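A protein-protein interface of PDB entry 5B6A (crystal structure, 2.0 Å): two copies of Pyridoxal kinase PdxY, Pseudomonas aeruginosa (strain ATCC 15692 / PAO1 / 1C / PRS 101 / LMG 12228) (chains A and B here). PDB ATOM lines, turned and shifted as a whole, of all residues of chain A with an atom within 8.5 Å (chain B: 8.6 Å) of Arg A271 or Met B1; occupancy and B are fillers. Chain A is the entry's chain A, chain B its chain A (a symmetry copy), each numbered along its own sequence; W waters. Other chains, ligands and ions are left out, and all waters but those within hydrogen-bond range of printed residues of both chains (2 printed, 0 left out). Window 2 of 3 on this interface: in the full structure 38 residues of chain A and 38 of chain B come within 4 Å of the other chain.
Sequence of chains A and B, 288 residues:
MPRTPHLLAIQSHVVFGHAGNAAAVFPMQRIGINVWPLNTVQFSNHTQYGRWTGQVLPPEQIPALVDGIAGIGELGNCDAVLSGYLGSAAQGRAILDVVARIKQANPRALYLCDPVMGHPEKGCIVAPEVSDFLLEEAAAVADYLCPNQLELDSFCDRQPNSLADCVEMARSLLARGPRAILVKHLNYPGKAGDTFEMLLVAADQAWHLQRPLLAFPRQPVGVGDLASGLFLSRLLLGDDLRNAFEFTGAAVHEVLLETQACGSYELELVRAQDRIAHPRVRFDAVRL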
ATOM      1  N   HIS A  18     -10.346 -27.786  10.220  1.00  0.00           N
ATOM      2  CA  HIS A  18     -10.293 -27.022   8.965  1.00  0.00           C
ATOM      3  C   HIS A  18     -11.532 -27.217   8.131  1.00  0.00           C
ATOM      4  O   HIS A  18     -11.856 -28.343   7.727  1.00  0.00           O
ATOM      5  CB  HIS A  18      -9.025 -27.380   8.158  1.00  0.00           C
ATOM      6  CG  HIS A  18      -7.766 -27.254   8.955  1.00  0.00           C
ATOM      7  ND1 HIS A  18      -7.216 -26.032   9.287  1.00  0.00           N
ATOM      8  CD2 HIS A  18      -6.987 -28.191   9.546  1.00  0.00           C
ATOM      9  CE1 HIS A  18      -6.135 -26.225  10.024  1.00  0.00           C
ATOM     10  NE2 HIS A  18      -5.975 -27.527  10.190  1.00  0.00           N
ATOM     11  N   PHE A  26      -5.051 -19.942   5.634  1.00  0.00           N
ATOM     12  CA  PHE A  26      -3.627 -20.228   5.782  1.00  0.00           C
ATOM     13  C   PHE A  26      -2.933 -20.644   4.448  1.00  0.00           C
ATOM     14  O   PHE A  26      -1.887 -20.071   4.105  1.00  0.00           O
ATOM     15  CB  PHE A  26      -3.319 -21.208   6.940  1.00  0.00           C
ATOM     16  CG  PHE A  26      -1.893 -21.688   6.927  1.00  0.00           C
ATOM     17  CD1 PHE A  26      -0.849 -20.811   7.247  1.00  0.00           C
ATOM     18  CD2 PHE A  26      -1.580 -22.997   6.520  1.00  0.00           C
ATOM     19  CE1 PHE A  26       0.482 -21.233   7.188  1.00  0.00           C
ATOM     20  CE2 PHE A  26      -0.255 -23.424   6.467  1.00  0.00           C
ATOM     21  CZ  PHE A  26       0.777 -22.543   6.813  1.00  0.00           C
ATOM     22  N   GLU A 254      -0.804 -32.952  -2.272  1.00  0.00           N
ATOM     23  CA  GLU A 254       0.217 -32.912  -1.203  1.00  0.00           C
ATOM     24  C   GLU A 254      -0.424 -32.852   0.186  1.00  0.00           C
ATOM     25  O   GLU A 254      -0.042 -33.597   1.083  1.00  0.00           O
ATOM     26  CB  GLU A 254       1.204 -31.754  -1.396  1.00  0.00           C
ATOM     27  CG  GLU A 254       2.097 -31.863  -2.633  1.00  0.00           C
ATOM     28  CD  GLU A 254       3.264 -32.844  -2.501  1.00  0.00           C
ATOM     29  OE1 GLU A 254       3.417 -33.523  -1.453  1.00  0.00           O
ATOM     30  OE2 GLU A 254       4.060 -32.926  -3.465  1.00  0.00           O
ATOM     31  N   VAL A 255      -1.429 -31.999   0.356  1.00  0.00           N
ATOM     32  CA  VAL A 255      -2.120 -31.912   1.654  1.00  0.00           C
ATOM     33  C   VAL A 255      -2.728 -33.267   2.020  1.00  0.00           C
ATOM     34  O   VAL A 255      -2.539 -33.750   3.136  1.00  0.00           O
ATOM     35  CB  VAL A 255      -3.223 -30.826   1.667  1.00  0.00           C
ATOM     36  CG1 VAL A 255      -4.024 -30.904   2.953  1.00  0.00           C
ATOM     37  CG2 VAL A 255      -2.609 -29.445   1.504  1.00  0.00           C
ATOM     38  N   GLU A 258      -0.148 -35.914   2.979  1.00  0.00           N
ATOM     39  CA  GLU A 258       0.306 -35.679   4.359  1.00  0.00           C
ATOM     40  C   GLU A 258      -0.793 -36.066   5.354  1.00  0.00           C
ATOM     41  O   GLU A 258      -0.507 -36.712   6.364  1.00  0.00           O
ATOM     42  CB  GLU A 258       0.744 -34.216   4.570  1.00  0.00           C
ATOM     43  CG  GLU A 258       1.328 -33.896   5.947  1.00  0.00           C
ATOM     44  CD  GLU A 258       2.696 -34.527   6.183  1.00  0.00           C
ATOM     45  OE1 GLU A 258       3.446 -34.721   5.202  1.00  0.00           O
ATOM     46  OE2 GLU A 258       3.016 -34.841   7.347  1.00  0.00           O
ATOM     47  N   THR A 259      -2.035 -35.675   5.052  1.00  0.00           N
ATOM     48  CA  THR A 259      -3.188 -36.036   5.892  1.00  0.00           C
ATOM     49  C   THR A 259      -3.312 -37.558   6.040  1.00  0.00           C
ATOM     50  O   THR A 259      -3.456 -38.067   7.160  1.00  0.00           O
ATOM     51  CB  THR A 259      -4.500 -35.414   5.378  1.00  0.00           C
ATOM     52  OG1 THR A 259      -4.308 -34.001   5.205  1.00  0.00           O
ATOM     53  CG2 THR A 259      -5.653 -35.639   6.380  1.00  0.00           C
ATOM     54  N   ALA A 261      -0.874 -39.872   5.437  1.00  0.00           N
ATOM     55  CA  ALA A 261       0.322 -40.432   6.086  1.00  0.00           C
ATOM     56  C   ALA A 261       0.301 -40.240   7.608  1.00  0.00           C
ATOM     57  O   ALA A 261       0.888 -41.035   8.328  1.00  0.00           O
ATOM     58  CB  ALA A 261       1.592 -39.859   5.482  1.00  0.00           C
ATOM     59  N   CYS A 262      -0.395 -39.197   8.082  1.00  0.00           N
ATOM     60  CA  CYS A 262      -0.580 -38.949   9.527  1.00  0.00           C
ATOM     61  C   CYS A 262      -1.723 -39.732  10.195  1.00  0.00           C
ATOM     62  O   CYS A 262      -1.822 -39.747  11.426  1.00  0.00           O
ATOM     63  CB  CYS A 262      -0.758 -37.454   9.802  1.00  0.00           C
ATOM     64  SG  CYS A 262       0.744 -36.495   9.537  1.00  0.00           S
ATOM     65  N   SER A 264      -4.834 -38.855   9.902  1.00  0.00           N
ATOM     66  CA  SER A 264      -5.691 -37.762  10.418  1.00  0.00           C
ATOM     67  C   SER A 264      -7.000 -37.604   9.664  1.00  0.00           C
ATOM     68  O   SER A 264      -7.066 -37.823   8.454  1.00  0.00           O
ATOM     69  CB  SER A 264      -4.969 -36.419  10.360  1.00  0.00           C
ATOM     70  OG  SER A 264      -3.741 -36.473  11.029  1.00  0.00           O
ATOM     71  N   LEU A 267      -7.405 -32.010   7.830  1.00  0.00           N
ATOM     72  CA  LEU A 267      -6.340 -31.666   6.870  1.00  0.00           C
ATOM     73  C   LEU A 267      -5.056 -31.166   7.551  1.00  0.00           C
ATOM     74  O   LEU A 267      -5.101 -30.234   8.367  1.00  0.00           O
ATOM     75  CB  LEU A 267      -6.851 -30.591   5.909  1.00  0.00           C
ATOM     76  CG  LEU A 267      -7.467 -30.893   4.531  1.00  0.00           C
ATOM     77  CD1 LEU A 267      -7.936 -32.313   4.309  1.00  0.00           C
ATOM     78  CD2 LEU A 267      -8.536 -29.867   4.232  1.00  0.00           C
ATOM     79  N   GLU A 268      -3.923 -31.773   7.184  1.00  0.00           N
ATOM     80  CA  GLU A 268      -2.613 -31.458   7.766  1.00  0.00           C
ATOM     81  C   GLU A 268      -1.938 -30.287   7.057  1.00  0.00           C
ATOM     82  O   GLU A 268      -0.842 -30.402   6.497  1.00  0.00           O
ATOM     83  CB  GLU A 268      -1.723 -32.711   7.793  1.00  0.00           C
ATOM     84  CG  GLU A 268      -2.226 -33.781   8.756  1.00  0.00           C
ATOM     85  CD  GLU A 268      -1.860 -33.518  10.218  1.00  0.00           C
ATOM     86  OE1 GLU A 268      -1.126 -32.550  10.507  1.00  0.00           O
ATOM     87  OE2 GLU A 268      -2.304 -34.302  11.088  1.00  0.00           O
ATOM     88  N   LEU A 269      -2.603 -29.137   7.140  1.00  0.00           N
ATOM     89  CA  LEU A 269      -2.245 -27.929   6.407  1.00  0.00           C
ATOM     90  C   LEU A 269      -0.875 -27.366   6.812  1.00  0.00           C
ATOM     91  O   LEU A 269      -0.039 -27.062   5.960  1.00  0.00           O
ATOM     92  CB  LEU A 269      -3.360 -26.886   6.634  1.00  0.00           C
ATOM     93  CG  LEU A 269      -4.437 -26.560   5.588  1.00  0.00           C
ATOM     94  CD1 LEU A 269      -4.861 -27.688   4.665  1.00  0.00           C
ATOM     95  CD2 LEU A 269      -5.629 -25.831   6.215  1.00  0.00           C
ATOM     96  N   VAL A 270      -0.660 -27.239   8.121  1.00  0.00           N
ATOM     97  CA  VAL A 270       0.610 -26.751   8.685  1.00  0.00           C
ATOM     98  C   VAL A 270       1.766 -27.702   8.370  1.00  0.00           C
ATOM     99  O   VAL A 270       2.803 -27.268   7.872  1.00  0.00           O
ATOM    100  CB  VAL A 270       0.479 -26.409  10.199  1.00  0.00           C
ATOM    101  CG1 VAL A 270       1.829 -26.091  10.820  1.00  0.00           C
ATOM    102  CG2 VAL A 270      -0.451 -25.216  10.384  1.00  0.00           C
ATOM    103  N   ARG A 271       1.591 -28.989   8.643  1.00  0.00           N
ATOM    104  CA  ARG A 271       2.620 -29.992   8.317  1.00  0.00           C
ATOM    105  C   ARG A 271       2.998 -30.041   6.832  1.00  0.00           C
ATOM    106  O   ARG A 271       4.155 -30.266   6.504  1.00  0.00           O
ATOM    107  CB  ARG A 271       2.179 -31.381   8.751  1.00  0.00           C
ATOM    108  CG  ARG A 271       2.501 -31.679  10.193  1.00  0.00           C
ATOM    109  CD  ARG A 271       2.213 -33.120  10.560  1.00  0.00           C
ATOM    110  NE  ARG A 271       3.319 -34.011  10.238  1.00  0.00           N
ATOM    111  CZ  ARG A 271       4.379 -34.233  11.017  1.00  0.00           C
ATOM    112  NH1 ARG A 271       4.519 -33.636  12.200  1.00  0.00           N
ATOM    113  NH2 ARG A 271       5.309 -35.074  10.607  1.00  0.00           N
ATOM    114  N   ALA A 272       2.026 -29.822   5.947  1.00  0.00           N
ATOM    115  CA  ALA A 272       2.233 -29.966   4.503  1.00  0.00           C
ATOM    116  C   ALA A 272       2.585 -28.655   3.806  1.00  0.00           C
ATOM    117  O   ALA A 272       2.650 -28.617   2.586  1.00  0.00           O
ATOM    118  CB  ALA A 272       0.976 -30.548   3.867  1.00  0.00           C
ATOM    119  N   GLN A 273       2.816 -27.588   4.567  1.00  0.00           N
ATOM    120  CA  GLN A 273       2.842 -26.221   3.999  1.00  0.00           C
ATOM    121  C   GLN A 273       3.922 -25.950   2.934  1.00  0.00           C
ATOM    122  O   GLN A 273       3.687 -25.198   1.981  1.00  0.00           O
ATOM    123  CB  GLN A 273       2.930 -25.167   5.102  1.00  0.00           C
ATOM    124  CG  GLN A 273       4.231 -25.157   5.900  1.00  0.00           C
ATOM    125  CD  GLN A 273       4.193 -24.094   6.977  1.00  0.00           C
ATOM    126  OE1 GLN A 273       3.863 -24.385   8.129  1.00  0.00           O
ATOM    127  NE2 GLN A 273       4.508 -22.856   6.611  1.00  0.00           N
ATOM    128  N   ASP A 274       5.095 -26.556   3.098  1.00  0.00           N
ATOM    129  CA  ASP A 274       6.166 -26.381   2.111  1.00  0.00           C
ATOM    130  C   ASP A 274       5.777 -26.983   0.767  1.00  0.00           C
ATOM    131  O   ASP A 274       6.179 -26.482  -0.283  1.00  0.00           O
ATOM    132  CB  ASP A 274       7.493 -26.932   2.641  1.00  0.00           C
ATOM    133  CG  ASP A 274       7.995 -26.157   3.861  1.00  0.00           C
ATOM    134  OD1 ASP A 274       7.341 -25.160   4.282  1.00  0.00           O
ATOM    135  OD2 ASP A 274       9.044 -26.543   4.404  1.00  0.00           O
ATOM    136  N   ARG A 275       4.941 -28.017   0.816  1.00  0.00           N
ATOM    137  CA  ARG A 275       4.488 -28.712  -0.392  1.00  0.00           C
ATOM    138  C   ARG A 275       3.159 -28.164  -0.919  1.00  0.00           C
ATOM    139  O   ARG A 275       2.723 -28.536  -2.011  1.00  0.00           O
ATOM    140  CB  ARG A 275       4.457 -30.225  -0.160  1.00  0.00           C
ATOM    141  CG  ARG A 275       5.832 -30.875  -0.294  1.00  0.00           C
ATOM    142  CD  ARG A 275       6.027 -31.982   0.729  1.00  0.00           C
ATOM    143  NE  ARG A 275       7.302 -32.675   0.520  1.00  0.00           N
ATOM    144  CZ  ARG A 275       7.725 -33.751   1.192  1.00  0.00           C
ATOM    145  NH1 ARG A 275       6.984 -34.309   2.151  1.00  0.00           N
ATOM    146  NH2 ARG A 275       8.903 -34.283   0.895  1.00  0.00           N
ATOM    147  N   ILE A 276       2.522 -27.276  -0.147  1.00  0.00           N
ATOM    148  CA  ILE A 276       1.496 -26.386  -0.694  1.00  0.00           C
ATOM    149  C   ILE A 276       2.196 -25.326  -1.545  1.00  0.00           C
ATOM    150  O   ILE A 276       1.813 -25.127  -2.704  1.00  0.00           O
ATOM    151  CB  ILE A 276       0.612 -25.706   0.395  1.00  0.00           C
ATOM    152  CG1 ILE A 276      -0.151 -26.763   1.199  1.00  0.00           C
ATOM    153  CG2 ILE A 276      -0.339 -24.694  -0.242  1.00  0.00           C
ATOM    154  CD1 ILE A 276      -0.944 -26.245   2.398  1.00  0.00           C
ATOM    155  N   MET B   1      10.597 -36.089  11.321  1.00  0.00           N
ATOM    156  CA  MET B   1      10.099 -34.793  11.873  1.00  0.00           C
ATOM    157  C   MET B   1       9.054 -35.006  12.993  1.00  0.00           C
ATOM    158  O   MET B   1       8.100 -35.772  12.808  1.00  0.00           O
ATOM    159  CB  MET B   1       9.586 -33.867  10.749  1.00  0.00           C
ATOM    160  CG  MET B   1       8.511 -34.438   9.829  1.00  0.00           C
ATOM    161  SD  MET B   1       9.030 -35.795   8.754  1.00  0.00           S
ATOM    162  CE  MET B   1       7.469 -36.285   8.019  1.00  0.00           C
ATOM    163  N   PRO B   2       9.247 -34.342  14.163  1.00  0.00           N
ATOM    164  CA  PRO B   2       8.400 -34.555  15.353  1.00  0.00           C
ATOM    165  C   PRO B   2       6.966 -34.037  15.181  1.00  0.00           C
ATOM    166  O   PRO B   2       6.695 -33.299  14.227  1.00  0.00           O
ATOM    167  CB  PRO B   2       9.125 -33.760  16.443  1.00  0.00           C
ATOM    168  CG  PRO B   2       9.860 -32.695  15.709  1.00  0.00           C
ATOM    169  CD  PRO B   2      10.290 -33.326  14.418  1.00  0.00           C
ATOM    170  N   ARG B   3       6.071 -34.420  16.095  1.00  0.00           N
ATOM    171  CA  ARG B   3       4.663 -34.008  16.029  1.00  0.00           C
ATOM    172  C   ARG B   3       4.498 -32.483  16.079  1.00  0.00           C
ATOM    173  O   ARG B   3       5.251 -31.775  16.763  1.00  0.00           O
ATOM    174  CB  ARG B   3       3.790 -34.718  17.088  1.00  0.00           C
ATOM    175  CG  ARG B   3       3.736 -34.063  18.461  1.00  0.00           C
ATOM    176  CD  ARG B   3       2.765 -34.767  19.400  1.00  0.00           C
ATOM    177  NE  ARG B   3       1.391 -34.250  19.351  1.00  0.00           N
ATOM    178  CZ  ARG B   3       0.944 -33.173  20.004  1.00  0.00           C
ATOM    179  NH1 ARG B   3       1.753 -32.435  20.756  1.00  0.00           N
ATOM    180  NH2 ARG B   3      -0.329 -32.817  19.897  1.00  0.00           N
ATOM    181  N   THR B   4       3.519 -31.999  15.324  1.00  0.00           N
ATOM    182  CA  THR B   4       3.223 -30.574  15.246  1.00  0.00           C
ATOM    183  C   THR B   4       2.483 -30.154  16.512  1.00  0.00           C
ATOM    184  O   THR B   4       1.474 -30.785  16.873  1.00  0.00           O
ATOM    185  CB  THR B   4       2.431 -30.254  13.967  1.00  0.00           C
ATOM    186  OG1 THR B   4       3.157 -30.781  12.853  1.00  0.00           O
ATOM    187  CG2 THR B   4       2.275 -28.754  13.768  1.00  0.00           C
ATOM    188  N   PRO B   5       2.997 -29.114  17.214  1.00  0.00           N
ATOM    189  CA  PRO B   5       2.282 -28.679  18.420  1.00  0.00           C
ATOM    190  C   PRO B   5       0.945 -27.991  18.086  1.00  0.00           C
ATOM    191  O   PRO B   5       0.726 -27.544  16.947  1.00  0.00           O
ATOM    192  CB  PRO B   5       3.281 -27.719  19.119  1.00  0.00           C
ATOM    193  CG  PRO B   5       4.596 -27.952  18.435  1.00  0.00           C
ATOM    194  CD  PRO B   5       4.267 -28.379  17.033  1.00  0.00           C
ATOM    195  N   HIS B   6       0.051 -27.976  19.071  1.00  0.00           N
ATOM    196  CA  HIS B   6      -1.265 -27.343  18.946  1.00  0.00           C
ATOM    197  C   HIS B   6      -1.373 -26.209  19.960  1.00  0.00           C
ATOM    198  O   HIS B   6      -1.013 -26.368  21.129  1.00  0.00           O
ATOM    199  CB  HIS B   6      -2.402 -28.341  19.225  1.00  0.00           C
ATOM    200  CG  HIS B   6      -2.616 -29.359  18.151  1.00  0.00           C
ATOM    201  ND1 HIS B   6      -1.849 -30.497  18.042  1.00  0.00           N
ATOM    202  CD2 HIS B   6      -3.546 -29.442  17.172  1.00  0.00           C
ATOM    203  CE1 HIS B   6      -2.276 -31.223  17.026  1.00  0.00           C
ATOM    204  NE2 HIS B   6      -3.312 -30.611  16.489  1.00  0.00           N
ATOM    205  N   GLN B  29       1.529 -20.402  12.522  1.00  0.00           N
ATOM    206  CA  GLN B  29       1.312 -21.513  11.582  1.00  0.00           C
ATOM    207  C   GLN B  29       2.511 -21.664  10.636  1.00  0.00           C
ATOM    208  O   GLN B  29       2.962 -22.794  10.356  1.00  0.00           O
ATOM    209  CB  GLN B  29       0.023 -21.313  10.749  1.00  0.00           C
ATOM    210  CG  GLN B  29      -1.283 -21.255  11.549  1.00  0.00           C
ATOM    211  CD  GLN B  29      -2.464 -20.795  10.712  1.00  0.00           C
ATOM    212  OE1 GLN B  29      -2.416 -19.765  10.044  1.00  0.00           O
ATOM    213  NE2 GLN B  29      -3.537 -21.556  10.759  1.00  0.00           N
ATOM    214  N   ILE B  31       5.621 -21.079  11.092  1.00  0.00           N
ATOM    215  CA  ILE B  31       6.827 -21.660  11.704  1.00  0.00           C
ATOM    216  C   ILE B  31       6.545 -23.058  12.288  1.00  0.00           C
ATOM    217  O   ILE B  31       7.358 -23.605  13.017  1.00  0.00           O
ATOM    218  CB  ILE B  31       7.532 -20.700  12.726  1.00  0.00           C
ATOM    219  CG1 ILE B  31       6.685 -20.460  13.993  1.00  0.00           C
ATOM    220  CG2 ILE B  31       7.895 -19.376  12.061  1.00  0.00           C
ATOM    221  CD1 ILE B  31       7.542 -20.122  15.205  1.00  0.00           C
ATOM    222  N   GLY B  32       5.369 -23.612  11.989  1.00  0.00           N
ATOM    223  CA  GLY B  32       5.086 -25.015  12.297  1.00  0.00           C
ATOM    224  C   GLY B  32       4.164 -25.299  13.468  1.00  0.00           C
ATOM    225  O   GLY B  32       4.263 -26.359  14.062  1.00  0.00           O
ATOM    226  N   ILE B  33       3.255 -24.374  13.795  1.00  0.00           N
ATOM    227  CA  ILE B  33       2.253 -24.595  14.871  1.00  0.00           C
ATOM    228  C   ILE B  33       0.837 -24.774  14.299  1.00  0.00           C
ATOM    229  O   ILE B  33       0.410 -23.956  13.494  1.00  0.00           O
ATOM    230  CB  ILE B  33       2.252 -23.410  15.901  1.00  0.00           C
ATOM    231  CG1 ILE B  33       3.686 -23.084  16.404  1.00  0.00           C
ATOM    232  CG2 ILE B  33       1.278 -23.657  17.056  1.00  0.00           C
ATOM    233  CD1 ILE B  33       4.398 -24.188  17.193  1.00  0.00           C
ATOM    234  N   ASN B  34       0.121 -25.834  14.696  1.00  0.00           N
ATOM    235  CA  ASN B  34      -1.330 -25.932  14.441  1.00  0.00           C
ATOM    236  C   ASN B  34      -2.020 -24.966  15.392  1.00  0.00           C
ATOM    237  O   ASN B  34      -2.081 -25.240  16.600  1.00  0.00           O
ATOM    238  CB  ASN B  34      -1.882 -27.331  14.730  1.00  0.00           C
ATOM    239  CG  ASN B  34      -1.410 -28.376  13.745  1.00  0.00           C
ATOM    240  OD1 ASN B  34      -1.438 -28.160  12.531  1.00  0.00           O
ATOM    241  ND2 ASN B  34      -1.007 -29.540  14.267  1.00  0.00           N
HETATM  242  O   HOH W   1      -0.841 -29.761  10.114  1.00  0.00           O
HETATM  243  O   HOH W   2       1.618 -34.167  14.060  1.00  0.00           O
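O of Pro B2 sits at hydrogen-bond distance from NH1 of Arg A271, 3.0 Å away.
The side-chain amide oxygen of Gln A273 lies close to the backbone carbonyl oxygen of Gln B29.
The side-chain hydroxyl of Thr B4 sits close to the guanidinium group of Arg A271, at 3.2 Å.
The guanidinium group (NE) of Arg A271 is in salt-bridge range of the side-chain carboxylate (OE2) of Glu A258 (3.0 Å).
A ring nitrogen (ND1) of His B6 sits at hydrogen-bond distance from the guanidinium group (NH2) of Arg B3, at 3.3 Å.
N of Asn B34 sits at hydrogen-bond distance from O of Pro B5 (2.9 Å).
NE of Arg A271 is in hydrogen-bond range of SG of Cys A262, 3.6 Å away.
The side-chain amide oxygen of Gln A273 lies close to the backbone carbonyl oxygen of Val A270 (3.1 Å).
A ring nitrogen (NE2) of His B6 is in hydrogen-bond range of the side-chain amide nitrogen (ND2) of Asn B34 (3.4 Å).
Among the printed residues, pairs that only touch across the chains: Phe A26 with Gln B29, Val A270 with Thr B4, Val A270 with Gln B29, Val A270 with Gly B32, Val A270 with Ile B33, Val A270 with Asn B34, Arg A271 with Met B1 and Arg A271 with Arg B3.
His A18 touches none of the printed residues of chain B.
Arg A271 touches just these residues of chain B: Met B1, Pro B2, Arg B3 and Thr B4.
No residue of chain B comes within 4 Å of Ala A272.
Of the printed residues of chain A, Thr B4 touches Val A270 (3.998 Å) and Arg A271 (2.9 Å).
Ile B31 touches none of the printed residues of chain A.
Printed residues of chain A within 4 Å of Asn B34: Val A270 (3.5 Å).
The nearest residue of chain B that does not touch Arg A271 is Asn B34 (5.0 Å).
The nearest residue of chain A that does not touch Met B1 is Glu A258 (4.7 Å).
Of the 19 printed residues of chain A, 4 touch a printed residue of chain B.
Hydrophobic or aromatic side chains of chain A that line the printed part of chain B: Phe A26 and Val A270.
Of the 11 printed residues of chain B, 8 touch a printed residue of chain A.
Among the printed residues, 11 pairs touch across the chains.
No position is printed for both chains.
Water W1 lies within hydrogen-bond range of OE1 of Glu A268, N of Arg A271, OD1 of Asn B34 and N of Val A270.
Water W2 bridges the backbone NH of Thr B4 (3.1 Å) and the guanidinium group of Arg A271 (3.5 Å).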
